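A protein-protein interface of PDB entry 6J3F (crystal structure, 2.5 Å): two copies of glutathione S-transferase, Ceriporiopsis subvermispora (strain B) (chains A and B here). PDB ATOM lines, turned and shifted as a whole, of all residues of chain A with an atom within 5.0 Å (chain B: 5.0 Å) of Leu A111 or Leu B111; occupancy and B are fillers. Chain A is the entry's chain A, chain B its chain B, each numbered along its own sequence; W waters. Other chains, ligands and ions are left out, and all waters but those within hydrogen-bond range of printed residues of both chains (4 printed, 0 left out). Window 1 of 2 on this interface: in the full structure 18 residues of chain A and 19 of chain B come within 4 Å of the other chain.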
ATOM      1  N   GLU A 107     -22.668  -3.832 -25.652  1.00  0.00           N
ATOM      2  CA  GLU A 107     -23.959  -4.294 -25.147  1.00  0.00           C
ATOM      3  C   GLU A 107     -23.899  -5.746 -24.676  1.00  0.00           C
ATOM      4  O   GLU A 107     -24.814  -6.198 -23.979  1.00  0.00           O
ATOM      5  CB  GLU A 107     -25.066  -4.095 -26.207  1.00  0.00           C
ATOM      6  CG  GLU A 107     -24.883  -4.829 -27.543  1.00  0.00           C
ATOM      7  CD  GLU A 107     -23.669  -4.354 -28.350  1.00  0.00           C
ATOM      8  OE1 GLU A 107     -23.257  -5.068 -29.291  1.00  0.00           O
ATOM      9  OE2 GLU A 107     -23.121  -3.272 -28.043  1.00  0.00           O
ATOM     10  N   THR A 108     -22.833  -6.472 -25.017  1.00  0.00           N
ATOM     11  CA  THR A 108     -22.602  -7.818 -24.512  1.00  0.00           C
ATOM     12  C   THR A 108     -21.563  -7.855 -23.392  1.00  0.00           C
ATOM     13  O   THR A 108     -21.189  -8.950 -22.946  1.00  0.00           O
ATOM     14  CB  THR A 108     -22.176  -8.749 -25.656  1.00  0.00           C
ATOM     15  OG1 THR A 108     -20.759  -8.665 -25.868  1.00  0.00           O
ATOM     16  CG2 THR A 108     -22.878  -8.358 -26.929  1.00  0.00           C
ATOM     17  N   ASP A 109     -21.101  -6.691 -22.916  1.00  0.00           N
ATOM     18  CA  ASP A 109     -20.011  -6.679 -21.945  1.00  0.00           C
ATOM     19  C   ASP A 109     -20.418  -7.347 -20.646  1.00  0.00           C
ATOM     20  O   ASP A 109     -19.658  -8.137 -20.090  1.00  0.00           O
ATOM     21  CB  ASP A 109     -19.530  -5.259 -21.639  1.00  0.00           C
ATOM     22  CG  ASP A 109     -18.310  -5.259 -20.699  1.00  0.00           C
ATOM     23  OD1 ASP A 109     -18.478  -5.334 -19.453  1.00  0.00           O
ATOM     24  OD2 ASP A 109     -17.174  -5.226 -21.225  1.00  0.00           O
ATOM     25  N   ALA A 110     -21.595  -7.008 -20.118  1.00  0.00           N
ATOM     26  CA  ALA A 110     -21.987  -7.594 -18.844  1.00  0.00           C
ATOM     27  C   ALA A 110     -22.289  -9.088 -18.984  1.00  0.00           C
ATOM     28  O   ALA A 110     -21.926  -9.878 -18.097  1.00  0.00           O
ATOM     29  CB  ALA A 110     -23.177  -6.846 -18.258  1.00  0.00           C
ATOM     30  N   LEU A 111     -22.929  -9.495 -20.098  1.00  0.00           N
ATOM     31  CA  LEU A 111     -23.184 -10.913 -20.354  1.00  0.00           C
ATOM     32  C   LEU A 111     -21.890 -11.686 -20.551  1.00  0.00           C
ATOM     33  O   LEU A 111     -21.805 -12.847 -20.161  1.00  0.00           O
ATOM     34  CB  LEU A 111     -24.105 -11.098 -21.577  1.00  0.00           C
ATOM     35  CG  LEU A 111     -25.563 -10.668 -21.410  1.00  0.00           C
ATOM     36  CD1 LEU A 111     -26.192 -10.537 -22.779  1.00  0.00           C
ATOM     37  CD2 LEU A 111     -26.347 -11.669 -20.565  1.00  0.00           C
ATOM     38  N   HIS A 112     -20.863 -11.056 -21.120  1.00  0.00           N
ATOM     39  CA  HIS A 112     -19.539 -11.675 -21.116  1.00  0.00           C
ATOM     40  C   HIS A 112     -19.046 -11.933 -19.696  1.00  0.00           C
ATOM     41  O   HIS A 112     -18.425 -12.969 -19.435  1.00  0.00           O
ATOM     42  CB  HIS A 112     -18.524 -10.818 -21.875  1.00  0.00           C
ATOM     43  CG  HIS A 112     -18.338 -11.220 -23.309  1.00  0.00           C
ATOM     44  ND1 HIS A 112     -19.049 -10.655 -24.341  1.00  0.00           N
ATOM     45  CD2 HIS A 112     -17.522 -12.138 -23.878  1.00  0.00           C
ATOM     46  CE1 HIS A 112     -18.669 -11.195 -25.483  1.00  0.00           C
ATOM     47  NE2 HIS A 112     -17.745 -12.101 -25.231  1.00  0.00           N
ATOM     48  N   ALA A 113     -19.312 -11.014 -18.760  1.00  0.00           N
ATOM     49  CA  ALA A 113     -18.816 -11.233 -17.402  1.00  0.00           C
ATOM     50  C   ALA A 113     -19.609 -12.322 -16.699  1.00  0.00           C
ATOM     51  O   ALA A 113     -19.027 -13.127 -15.960  1.00  0.00           O
ATOM     52  CB  ALA A 113     -18.834  -9.947 -16.584  1.00  0.00           C
ATOM     53  N   ALA A 114     -20.918 -12.403 -16.943  1.00  0.00           N
ATOM     54  CA  ALA A 114     -21.645 -13.565 -16.455  1.00  0.00           C
ATOM     55  C   ALA A 114     -21.164 -14.844 -17.129  1.00  0.00           C
ATOM     56  O   ALA A 114     -21.153 -15.913 -16.496  1.00  0.00           O
ATOM     57  CB  ALA A 114     -23.140 -13.380 -16.659  1.00  0.00           C
ATOM     58  N   PHE A 115     -20.779 -14.772 -18.410  1.00  0.00           N
ATOM     59  CA  PHE A 115     -20.346 -15.990 -19.092  1.00  0.00           C
ATOM     60  C   PHE A 115     -19.056 -16.522 -18.479  1.00  0.00           C
ATOM     61  O   PHE A 115     -18.857 -17.743 -18.386  1.00  0.00           O
ATOM     62  CB  PHE A 115     -20.165 -15.740 -20.588  1.00  0.00           C
ATOM     63  CG  PHE A 115     -19.276 -16.755 -21.273  1.00  0.00           C
ATOM     64  CD1 PHE A 115     -19.813 -17.925 -21.799  1.00  0.00           C
ATOM     65  CD2 PHE A 115     -17.889 -16.556 -21.364  1.00  0.00           C
ATOM     66  CE1 PHE A 115     -18.992 -18.861 -22.413  1.00  0.00           C
ATOM     67  CE2 PHE A 115     -17.075 -17.477 -21.971  1.00  0.00           C
ATOM     68  CZ  PHE A 115     -17.629 -18.634 -22.509  1.00  0.00           C
ATOM     69  N   PHE A 199     -20.481 -17.587 -30.167  1.00  0.00           N
ATOM     70  CA  PHE A 199     -21.550 -17.119 -29.292  1.00  0.00           C
ATOM     71  C   PHE A 199     -22.396 -16.025 -29.940  1.00  0.00           C
ATOM     72  O   PHE A 199     -23.626 -16.024 -29.794  1.00  0.00           O
ATOM     73  CB  PHE A 199     -20.968 -16.664 -27.953  1.00  0.00           C
ATOM     74  CG  PHE A 199     -20.996 -17.754 -26.921  1.00  0.00           C
ATOM     75  CD1 PHE A 199     -20.004 -18.726 -26.893  1.00  0.00           C
ATOM     76  CD2 PHE A 199     -22.043 -17.852 -26.032  1.00  0.00           C
ATOM     77  CE1 PHE A 199     -20.034 -19.764 -25.958  1.00  0.00           C
ATOM     78  CE2 PHE A 199     -22.086 -18.894 -25.097  1.00  0.00           C
ATOM     79  CZ  PHE A 199     -21.075 -19.849 -25.058  1.00  0.00           C
ATOM     80  N   LEU A 200     -21.764 -15.080 -30.647  1.00  0.00           N
ATOM     81  CA  LEU A 200     -22.521 -14.007 -31.290  1.00  0.00           C
ATOM     82  C   LEU A 200     -23.208 -14.441 -32.577  1.00  0.00           C
ATOM     83  O   LEU A 200     -24.057 -13.697 -33.083  1.00  0.00           O
ATOM     84  CB  LEU A 200     -21.610 -12.826 -31.601  1.00  0.00           C
ATOM     85  CG  LEU A 200     -21.039 -12.174 -30.365  1.00  0.00           C
ATOM     86  CD1 LEU A 200     -20.252 -11.000 -30.824  1.00  0.00           C
ATOM     87  CD2 LEU A 200     -22.167 -11.752 -29.443  1.00  0.00           C
ATOM     88  N   ALA A 207     -15.943 -14.566 -25.659  1.00  0.00           N
ATOM     89  CA  ALA A 207     -16.522 -15.812 -25.163  1.00  0.00           C
ATOM     90  C   ALA A 207     -16.012 -17.000 -25.958  1.00  0.00           C
ATOM     91  O   ALA A 207     -15.695 -18.049 -25.381  1.00  0.00           O
ATOM     92  CB  ALA A 207     -18.056 -15.761 -25.202  1.00  0.00           C
ATOM     93  N   GLU B 107     -28.113 -11.951 -31.332  1.00  0.00           N
ATOM     94  CA  GLU B 107     -26.680 -12.038 -31.085  1.00  0.00           C
ATOM     95  C   GLU B 107     -26.357 -12.337 -29.629  1.00  0.00           C
ATOM     96  O   GLU B 107     -25.253 -12.813 -29.341  1.00  0.00           O
ATOM     97  CB  GLU B 107     -25.994 -10.735 -31.488  1.00  0.00           C
ATOM     98  CG  GLU B 107     -25.796 -10.588 -32.978  1.00  0.00           C
ATOM     99  CD  GLU B 107     -25.059  -9.312 -33.321  1.00  0.00           C
ATOM    100  OE1 GLU B 107     -24.546  -8.673 -32.381  1.00  0.00           O
ATOM    101  OE2 GLU B 107     -24.978  -8.958 -34.519  1.00  0.00           O
ATOM    102  N   THR B 108     -27.274 -12.035 -28.709  1.00  0.00           N
ATOM    103  CA  THR B 108     -27.071 -12.289 -27.290  1.00  0.00           C
ATOM    104  C   THR B 108     -27.776 -13.552 -26.815  1.00  0.00           C
ATOM    105  O   THR B 108     -27.914 -13.759 -25.602  1.00  0.00           O
ATOM    106  CB  THR B 108     -27.548 -11.094 -26.473  1.00  0.00           C
ATOM    107  OG1 THR B 108     -28.976 -11.052 -26.491  1.00  0.00           O
ATOM    108  CG2 THR B 108     -27.019  -9.844 -27.077  1.00  0.00           C
ATOM    109  N   ASP B 109     -28.231 -14.400 -27.738  1.00  0.00           N
ATOM    110  CA  ASP B 109     -29.059 -15.528 -27.331  1.00  0.00           C
ATOM    111  C   ASP B 109     -28.234 -16.566 -26.578  1.00  0.00           C
ATOM    112  O   ASP B 109     -28.602 -16.977 -25.470  1.00  0.00           O
ATOM    113  CB  ASP B 109     -29.760 -16.152 -28.548  1.00  0.00           C
ATOM    114  CG  ASP B 109     -30.780 -17.206 -28.150  1.00  0.00           C
ATOM    115  OD1 ASP B 109     -30.356 -18.346 -27.874  1.00  0.00           O
ATOM    116  OD2 ASP B 109     -31.993 -16.892 -28.098  1.00  0.00           O
ATOM    117  N   ALA B 110     -27.108 -16.994 -27.158  1.00  0.00           N
ATOM    118  CA  ALA B 110     -26.240 -17.956 -26.480  1.00  0.00           C
ATOM    119  C   ALA B 110     -25.754 -17.409 -25.140  1.00  0.00           C
ATOM    120  O   ALA B 110     -25.809 -18.110 -24.119  1.00  0.00           O
ATOM    121  CB  ALA B 110     -25.060 -18.326 -27.378  1.00  0.00           C
ATOM    122  N   LEU B 111     -25.284 -16.153 -25.126  1.00  0.00           N
ATOM    123  CA  LEU B 111     -24.864 -15.514 -23.879  1.00  0.00           C
ATOM    124  C   LEU B 111     -25.998 -15.445 -22.863  1.00  0.00           C
ATOM    125  O   LEU B 111     -25.751 -15.546 -21.658  1.00  0.00           O
ATOM    126  CB  LEU B 111     -24.319 -14.107 -24.147  1.00  0.00           C
ATOM    127  CG  LEU B 111     -22.888 -13.977 -24.713  1.00  0.00           C
ATOM    128  CD1 LEU B 111     -22.604 -12.560 -25.259  1.00  0.00           C
ATOM    129  CD2 LEU B 111     -21.844 -14.352 -23.675  1.00  0.00           C
ATOM    130  N   HIS B 112     -27.246 -15.279 -23.313  1.00  0.00           N
ATOM    131  CA  HIS B 112     -28.362 -15.357 -22.370  1.00  0.00           C
ATOM    132  C   HIS B 112     -28.473 -16.759 -21.768  1.00  0.00           C
ATOM    133  O   HIS B 112     -28.810 -16.915 -20.587  1.00  0.00           O
ATOM    134  CB  HIS B 112     -29.671 -14.952 -23.050  1.00  0.00           C
ATOM    135  CG  HIS B 112     -30.022 -13.495 -22.902  1.00  0.00           C
ATOM    136  ND1 HIS B 112     -29.541 -12.520 -23.750  1.00  0.00           N
ATOM    137  CD2 HIS B 112     -30.836 -12.859 -22.024  1.00  0.00           C
ATOM    138  CE1 HIS B 112     -30.022 -11.348 -23.385  1.00  0.00           C
ATOM    139  NE2 HIS B 112     -30.816 -11.525 -22.344  1.00  0.00           N
ATOM    140  N   ALA B 113     -28.179 -17.797 -22.556  1.00  0.00           N
ATOM    141  CA  ALA B 113     -28.267 -19.147 -22.014  1.00  0.00           C
ATOM    142  C   ALA B 113     -27.114 -19.417 -21.048  1.00  0.00           C
ATOM    143  O   ALA B 113     -27.310 -20.049 -20.005  1.00  0.00           O
ATOM    144  CB  ALA B 113     -28.303 -20.173 -23.148  1.00  0.00           C
ATOM    145  N   ALA B 114     -25.916 -18.919 -21.361  1.00  0.00           N
ATOM    146  CA  ALA B 114     -24.834 -18.916 -20.374  1.00  0.00           C
ATOM    147  C   ALA B 114     -25.220 -18.124 -19.130  1.00  0.00           C
ATOM    148  O   ALA B 114     -24.878 -18.512 -18.006  1.00  0.00           O
ATOM    149  CB  ALA B 114     -23.554 -18.342 -20.983  1.00  0.00           C
ATOM    150  N   PHE B 115     -25.951 -17.022 -19.305  1.00  0.00           N
ATOM    151  CA  PHE B 115     -26.279 -16.196 -18.147  1.00  0.00           C
ATOM    152  C   PHE B 115     -27.235 -16.928 -17.220  1.00  0.00           C
ATOM    153  O   PHE B 115     -27.142 -16.797 -15.993  1.00  0.00           O
ATOM    154  CB  PHE B 115     -26.869 -14.839 -18.575  1.00  0.00           C
ATOM    155  CG  PHE B 115     -27.673 -14.141 -17.481  1.00  0.00           C
ATOM    156  CD1 PHE B 115     -27.059 -13.267 -16.598  1.00  0.00           C
ATOM    157  CD2 PHE B 115     -29.047 -14.370 -17.339  1.00  0.00           C
ATOM    158  CE1 PHE B 115     -27.793 -12.627 -15.596  1.00  0.00           C
ATOM    159  CE2 PHE B 115     -29.777 -13.751 -16.329  1.00  0.00           C
ATOM    160  CZ  PHE B 115     -29.149 -12.870 -15.464  1.00  0.00           C
ATOM    161  N   PHE B 199     -28.472  -5.178 -18.432  1.00  0.00           N
ATOM    162  CA  PHE B 199     -27.350  -5.955 -18.940  1.00  0.00           C
ATOM    163  C   PHE B 199     -26.840  -5.419 -20.267  1.00  0.00           C
ATOM    164  O   PHE B 199     -25.627  -5.416 -20.509  1.00  0.00           O
ATOM    165  CB  PHE B 199     -27.743  -7.432 -19.046  1.00  0.00           C
ATOM    166  CG  PHE B 199     -27.285  -8.220 -17.875  1.00  0.00           C
ATOM    167  CD1 PHE B 199     -28.055  -8.281 -16.730  1.00  0.00           C
ATOM    168  CD2 PHE B 199     -26.033  -8.801 -17.876  1.00  0.00           C
ATOM    169  CE1 PHE B 199     -27.608  -8.947 -15.624  1.00  0.00           C
ATOM    170  CE2 PHE B 199     -25.577  -9.466 -16.768  1.00  0.00           C
ATOM    171  CZ  PHE B 199     -26.369  -9.553 -15.644  1.00  0.00           C
ATOM    172  N   LEU B 200     -27.741  -4.960 -21.136  1.00  0.00           N
ATOM    173  CA  LEU B 200     -27.341  -4.405 -22.423  1.00  0.00           C
ATOM    174  C   LEU B 200     -26.976  -2.929 -22.354  1.00  0.00           C
ATOM    175  O   LEU B 200     -26.465  -2.388 -23.338  1.00  0.00           O
ATOM    176  CB  LEU B 200     -28.455  -4.596 -23.448  1.00  0.00           C
ATOM    177  CG  LEU B 200     -28.925  -6.026 -23.537  1.00  0.00           C
ATOM    178  CD1 LEU B 200     -30.098  -6.030 -24.475  1.00  0.00           C
ATOM    179  CD2 LEU B 200     -27.803  -6.961 -24.018  1.00  0.00           C
ATOM    180  N   ALA B 207     -32.338 -10.972 -19.510  1.00  0.00           N
ATOM    181  CA  ALA B 207     -31.429 -11.143 -18.383  1.00  0.00           C
ATOM    182  C   ALA B 207     -31.840 -10.264 -17.210  1.00  0.00           C
ATOM    183  O   ALA B 207     -31.768 -10.692 -16.052  1.00  0.00           O
ATOM    184  CB  ALA B 207     -29.989 -10.853 -18.819  1.00  0.00           C
HETATM  185  O   HOH W   1     -24.603 -14.820 -27.570  1.00  0.00           O
HETATM  186  O   HOH W   2     -26.499 -16.258 -29.835  1.00  0.00           O
HETATM  187  O   HOH W   3     -23.122  -4.421 -21.041  1.00  0.00           O
HETATM  188  O   HOH W   4     -24.444  -7.564 -21.763  1.00  0.00           O
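A ring nitrogen (NE2) of His B112 lies within hydrogen-bond range of the backbone NH (N) of Ala B207 (3.3 Å). OG1 of Thr A108 lies within hydrogen-bond range of ND1 of His A112 (3.0 Å). A ring nitrogen (ND1) of His B112 lies within hydrogen-bond range of the backbone carbonyl oxygen of Thr B108 (2.8 Å).
Glu A107 touches Phe B199 (O to O, 3.6 Å). Glu A107 touches Leu B200 (O to CD2, 3.1 Å). CD2 of Phe B199 touches CB of Ala A110, at 3.5 Å. CD1 of Leu A111 touches CB of Thr B108 (3.97 Å). Leu B111 touches Leu A111. CD2 of Leu A111 touches CB of Phe B115, 3.8 Å away. N of Leu A111 touches CD2 of Phe B199, 3.9 Å away. CD1 of Phe B115 touches CB of Ala A114 (3.9 Å). Phe A199 touches Glu B107. Leu A200 touches Glu B107 (CD2 to O, 3.3 Å).
Of chain B, only Thr B108 (3.97 Å), Leu B111 (3.8 Å), His B112 (3.96 Å), Phe B115 (3.8 Å) and Phe B199 (3.9 Å) come within 4 Å of Leu A111. Leu B111 touches four residues of chain A. Of the printed residues of chain A, Glu B107 touches Phe A199 (3.6 Å) and Leu A200 (3.3 Å). Printed residues of chain A within 4 Å of Phe B199: Glu A107, Ala A110 and Leu A111. Ala A113 touches none of the printed residues of chain B. Ala B113 touches none of the printed residues of chain A. The nearest printed residue of chain B that does not touch Leu A111 is Leu B200 (4.1 Å). The nearest residue of chain A that does not touch Leu B111 is His A112 (4.1 Å). The nearest printed residue of chain B that does not touch Ala A114 is Phe B199 (4.6 Å).
Of the 12 printed residues of chain B, 9 touch a printed residue of chain A. Hydrophobic or aromatic side chains of chain B within 4 Å of the printed part of chain A: Ala B110, Leu B111, His B112, Ala B114, Phe B115, Phe B199 and Leu B200.
Glu A107 touches Phe B199, and with the chains exchanged Phe A199 touches Glu B107. Ala A110 touches Phe B199, and with the chains exchanged Phe A199 touches Ala B110. Leu B111 touches its own counterpart, Leu A111. Leu A111 touches Phe B199, and with the chains exchanged Phe A199 touches Leu B111. 12 positions are printed for both chains. Of the 16 pairs that touch across the chains among the printed residues, 15 have their exchanged pair printed and touching as well.
Water W4 lies within hydrogen-bond range of the backbone carbonyl oxygen (O) of Glu A107 (2.6 Å), the backbone carbonyl oxygen (O) of Phe B199 (2.8 Å), the backbone NH (N) of Leu A111 (3.0 Å) and the backbone NH (N) of Ala A110 (3.3 Å). Water W1 lies within hydrogen-bond range of O of Phe A199, O of Glu B107, N of Leu B111 and N of Ala B110. Water W3 bridges the backbone carbonyl oxygen (O) of Phe B199 (2.7 Å) and the backbone NH (N) of Ala A110 (3.1 Å). Water W2 lies within hydrogen-bond range of the backbone NH (N) of Ala B110 (2.8 Å), the backbone carbonyl oxygen (O) of Phe A199 (2.9 Å) and the backbone NH (N) of Asp B109 (3.3 Å).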
